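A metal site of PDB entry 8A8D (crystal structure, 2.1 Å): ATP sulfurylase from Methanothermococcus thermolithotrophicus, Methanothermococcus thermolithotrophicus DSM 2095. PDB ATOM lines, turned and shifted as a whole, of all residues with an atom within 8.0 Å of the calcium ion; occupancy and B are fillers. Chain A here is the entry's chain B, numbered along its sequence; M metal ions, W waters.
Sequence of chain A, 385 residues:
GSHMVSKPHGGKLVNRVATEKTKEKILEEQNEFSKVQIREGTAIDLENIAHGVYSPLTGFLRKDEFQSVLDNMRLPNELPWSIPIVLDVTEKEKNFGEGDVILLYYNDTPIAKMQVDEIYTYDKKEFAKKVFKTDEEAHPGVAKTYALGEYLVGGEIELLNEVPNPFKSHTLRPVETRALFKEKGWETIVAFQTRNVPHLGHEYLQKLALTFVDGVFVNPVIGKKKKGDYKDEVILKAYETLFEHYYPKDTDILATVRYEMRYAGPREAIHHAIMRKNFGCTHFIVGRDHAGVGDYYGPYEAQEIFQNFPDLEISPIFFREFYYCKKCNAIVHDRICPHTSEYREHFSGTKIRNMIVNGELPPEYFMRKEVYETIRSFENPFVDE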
ATOM      1  N   ASP A  88      16.998  26.722  -0.250  1.00  0.00           N
ATOM      2  CA  ASP A  88      17.227  27.061   1.148  1.00  0.00           C
ATOM      3  C   ASP A  88      16.216  28.105   1.604  1.00  0.00           C
ATOM      4  O   ASP A  88      15.895  29.036   0.867  1.00  0.00           O
ATOM      5  CB  ASP A  88      18.642  27.586   1.360  1.00  0.00           C
ATOM      6  CG  ASP A  88      18.904  28.860   0.596  1.00  0.00           C
ATOM      7  OD1 ASP A  88      18.812  28.847  -0.649  1.00  0.00           O
ATOM      8  OD2 ASP A  88      19.187  29.891   1.248  1.00  0.00           O
ATOM      9  N   THR A  90      14.984  30.274   5.423  1.00  0.00           N
ATOM     10  CA  THR A  90      15.174  30.512   6.841  1.00  0.00           C
ATOM     11  C   THR A  90      13.931  30.069   7.615  1.00  0.00           C
ATOM     12  O   THR A  90      12.912  29.682   7.037  1.00  0.00           O
ATOM     13  CB  THR A  90      15.460  31.986   7.116  1.00  0.00           C
ATOM     14  OG1 THR A  90      14.295  32.764   6.853  1.00  0.00           O
ATOM     15  CG2 THR A  90      16.606  32.486   6.259  1.00  0.00           C
ATOM     16  N   TYR A 122      21.606  20.935   7.855  1.00  0.00           N
ATOM     17  CA  TYR A 122      22.895  20.554   7.296  1.00  0.00           C
ATOM     18  C   TYR A 122      24.016  21.291   8.020  1.00  0.00           C
ATOM     19  O   TYR A 122      23.779  22.267   8.738  1.00  0.00           O
ATOM     20  CB  TYR A 122      22.947  20.853   5.791  1.00  0.00           C
ATOM     21  CG  TYR A 122      22.768  22.317   5.459  1.00  0.00           C
ATOM     22  CD1 TYR A 122      21.525  22.914   5.533  1.00  0.00           C
ATOM     23  CD2 TYR A 122      23.854  23.105   5.077  1.00  0.00           C
ATOM     24  CE1 TYR A 122      21.354  24.260   5.227  1.00  0.00           C
ATOM     25  CE2 TYR A 122      23.698  24.436   4.776  1.00  0.00           C
ATOM     26  CZ  TYR A 122      22.448  25.012   4.847  1.00  0.00           C
ATOM     27  OH  TYR A 122      22.284  26.346   4.545  1.00  0.00           O
ATOM     28  N   LYS A 124      27.014  23.555   7.433  1.00  0.00           N
ATOM     29  CA  LYS A 124      27.523  24.526   6.424  1.00  0.00           C
ATOM     30  C   LYS A 124      29.037  24.366   6.190  1.00  0.00           C
ATOM     31  O   LYS A 124      29.467  24.607   5.059  1.00  0.00           O
ATOM     32  CB  LYS A 124      27.113  25.958   6.765  1.00  0.00           C
ATOM     33  CG  LYS A 124      27.527  26.453   8.142  1.00  0.00           C
ATOM     34  CD  LYS A 124      26.815  27.724   8.556  1.00  0.00           C
ATOM     35  CE  LYS A 124      27.656  28.612   9.456  1.00  0.00           C
ATOM     36  NZ  LYS A 124      28.273  27.842  10.559  1.00  0.00           N
ATOM     37  N   ALA A 143      31.368  31.619   0.951  1.00  0.00           N
ATOM     38  CA  ALA A 143      30.569  32.679   1.554  1.00  0.00           C
ATOM     39  C   ALA A 143      29.107  32.565   1.162  1.00  0.00           C
ATOM     40  O   ALA A 143      28.216  32.785   2.002  1.00  0.00           O
ATOM     41  CB  ALA A 143      31.123  34.049   1.156  1.00  0.00           C
ATOM     42  N   LYS A 144      28.823  32.213  -0.088  1.00  0.00           N
ATOM     43  CA  LYS A 144      27.438  32.058  -0.517  1.00  0.00           C
ATOM     44  C   LYS A 144      26.812  30.813   0.092  1.00  0.00           C
ATOM     45  O   LYS A 144      25.595  30.772   0.302  1.00  0.00           O
ATOM     46  CB  LYS A 144      27.361  32.010  -2.044  1.00  0.00           C
ATOM     47  CG  LYS A 144      27.136  33.381  -2.673  1.00  0.00           C
ATOM     48  CD  LYS A 144      27.900  33.563  -3.975  1.00  0.00           C
ATOM     49  CE  LYS A 144      27.494  32.520  -5.014  1.00  0.00           C
ATOM     50  NZ  LYS A 144      27.565  33.071  -6.398  1.00  0.00           N
ATOM     51  N   THR A 145      27.610  29.785   0.380  1.00  0.00           N
ATOM     52  CA  THR A 145      27.097  28.629   1.100  1.00  0.00           C
ATOM     53  C   THR A 145      26.686  29.013   2.520  1.00  0.00           C
ATOM     54  O   THR A 145      25.652  28.543   3.025  1.00  0.00           O
ATOM     55  CB  THR A 145      28.145  27.518   1.138  1.00  0.00           C
ATOM     56  OG1 THR A 145      28.599  27.231  -0.196  1.00  0.00           O
ATOM     57  CG2 THR A 145      27.575  26.256   1.764  1.00  0.00           C
ATOM     58  N   TYR A 146      27.480  29.859   3.181  1.00  0.00           N
ATOM     59  CA  TYR A 146      27.167  30.256   4.547  1.00  0.00           C
ATOM     60  C   TYR A 146      25.932  31.148   4.614  1.00  0.00           C
ATOM     61  O   TYR A 146      25.164  31.068   5.581  1.00  0.00           O
ATOM     62  CB  TYR A 146      28.376  30.960   5.168  1.00  0.00           C
ATOM     63  CG  TYR A 146      29.556  30.058   5.479  1.00  0.00           C
ATOM     64  CD1 TYR A 146      29.496  28.695   5.240  1.00  0.00           C
ATOM     65  CD2 TYR A 146      30.735  30.580   6.010  1.00  0.00           C
ATOM     66  CE1 TYR A 146      30.568  27.870   5.524  1.00  0.00           C
ATOM     67  CE2 TYR A 146      31.811  29.765   6.291  1.00  0.00           C
ATOM     68  CZ  TYR A 146      31.723  28.409   6.038  1.00  0.00           C
ATOM     69  OH  TYR A 146      32.785  27.588   6.321  1.00  0.00           O
ATOM     70  N   ALA A 147      25.731  31.984   3.606  1.00  0.00           N
ATOM     71  CA  ALA A 147      24.550  32.837   3.572  1.00  0.00           C
ATOM     72  C   ALA A 147      23.269  32.062   3.295  1.00  0.00           C
ATOM     73  O   ALA A 147      22.184  32.652   3.365  1.00  0.00           O
ATOM     74  CB  ALA A 147      24.725  33.934   2.514  1.00  0.00           C
ATOM     75  N   LEU A 148      23.358  30.768   2.996  1.00  0.00           N
ATOM     76  CA  LEU A 148      22.165  29.975   2.738  1.00  0.00           C
ATOM     77  C   LEU A 148      21.313  29.857   3.987  1.00  0.00           C
ATOM     78  O   LEU A 148      21.803  29.926   5.120  1.00  0.00           O
ATOM     79  CB  LEU A 148      22.547  28.584   2.236  1.00  0.00           C
ATOM     80  CG  LEU A 148      23.171  28.481   0.840  1.00  0.00           C
ATOM     81  CD1 LEU A 148      23.613  27.047   0.573  1.00  0.00           C
ATOM     82  CD2 LEU A 148      22.209  28.948  -0.232  1.00  0.00           C
ATOM     83  N   GLY A 149      20.009  29.679   3.776  1.00  0.00           N
ATOM     84  CA  GLY A 149      19.111  29.436   4.884  1.00  0.00           C
ATOM     85  C   GLY A 149      19.411  28.123   5.581  1.00  0.00           C
ATOM     86  O   GLY A 149      20.033  27.214   5.031  1.00  0.00           O
ATOM     87  N   GLU A 150      18.952  28.030   6.833  1.00  0.00           N
ATOM     88  CA  GLU A 150      19.293  26.890   7.677  1.00  0.00           C
ATOM     89  C   GLU A 150      18.564  25.624   7.263  1.00  0.00           C
ATOM     90  O   GLU A 150      18.979  24.524   7.667  1.00  0.00           O
ATOM     91  CB  GLU A 150      18.997  27.219   9.138  1.00  0.00           C
ATOM     92  CG  GLU A 150      20.029  28.109   9.812  1.00  0.00           C
ATOM     93  CD  GLU A 150      20.294  29.393   9.045  1.00  0.00           C
ATOM     94  OE1 GLU A 150      21.458  29.629   8.637  1.00  0.00           O
ATOM     95  OE2 GLU A 150      19.335  30.171   8.830  1.00  0.00           O
ATOM     96  N   TYR A 151      17.490  25.734   6.488  1.00  0.00           N
ATOM     97  CA  TYR A 151      16.709  24.582   6.048  1.00  0.00           C
ATOM     98  C   TYR A 151      16.841  24.435   4.537  1.00  0.00           C
ATOM     99  O   TYR A 151      16.685  25.413   3.801  1.00  0.00           O
ATOM    100  CB  TYR A 151      15.228  24.734   6.411  1.00  0.00           C
ATOM    101  CG  TYR A 151      14.951  24.882   7.886  1.00  0.00           C
ATOM    102  CD1 TYR A 151      14.910  26.127   8.495  1.00  0.00           C
ATOM    103  CD2 TYR A 151      14.709  23.764   8.676  1.00  0.00           C
ATOM    104  CE1 TYR A 151      14.647  26.264   9.838  1.00  0.00           C
ATOM    105  CE2 TYR A 151      14.449  23.879  10.026  1.00  0.00           C
ATOM    106  CZ  TYR A 151      14.415  25.133  10.600  1.00  0.00           C
ATOM    107  OH  TYR A 151      14.158  25.257  11.948  1.00  0.00           O
HETATM  108 CA    CA M   1      23.310  30.130   7.140  1.00  0.00          CA
HETATM  109  O   HOH W   1      22.111  32.120   7.570  1.00  0.00           O
HETATM  110  O   HOH W   2      24.377  28.439   5.933  1.00  0.00           O
HETATM  111  O   HOH W   3      24.447  30.507   9.180  1.00  0.00           O
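The nearest printed residue that does not touch the calcium ion is Ala 147 (4.3 Å).
The calcium ion is bound by water W2 (2.3 Å). Water W1 is bound to the calcium ion (2.4 Å). Water W3 is bound to the calcium ion (2.4 Å). OE1 of Glu 150 is bound to the calcium ion, 2.4 Å away. The calcium ion is bound by the backbone carbonyl oxygen (O) of Leu 148, at 2.5 Å. The calcium ion is bound by the backbone carbonyl oxygen (O) of Tyr 146 (2.6 Å).
Water W2 bridges the backbone carbonyl oxygen of Thr 145 (3.2 Å) and the side-chain hydroxyl of Tyr 122 (3.3 Å).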
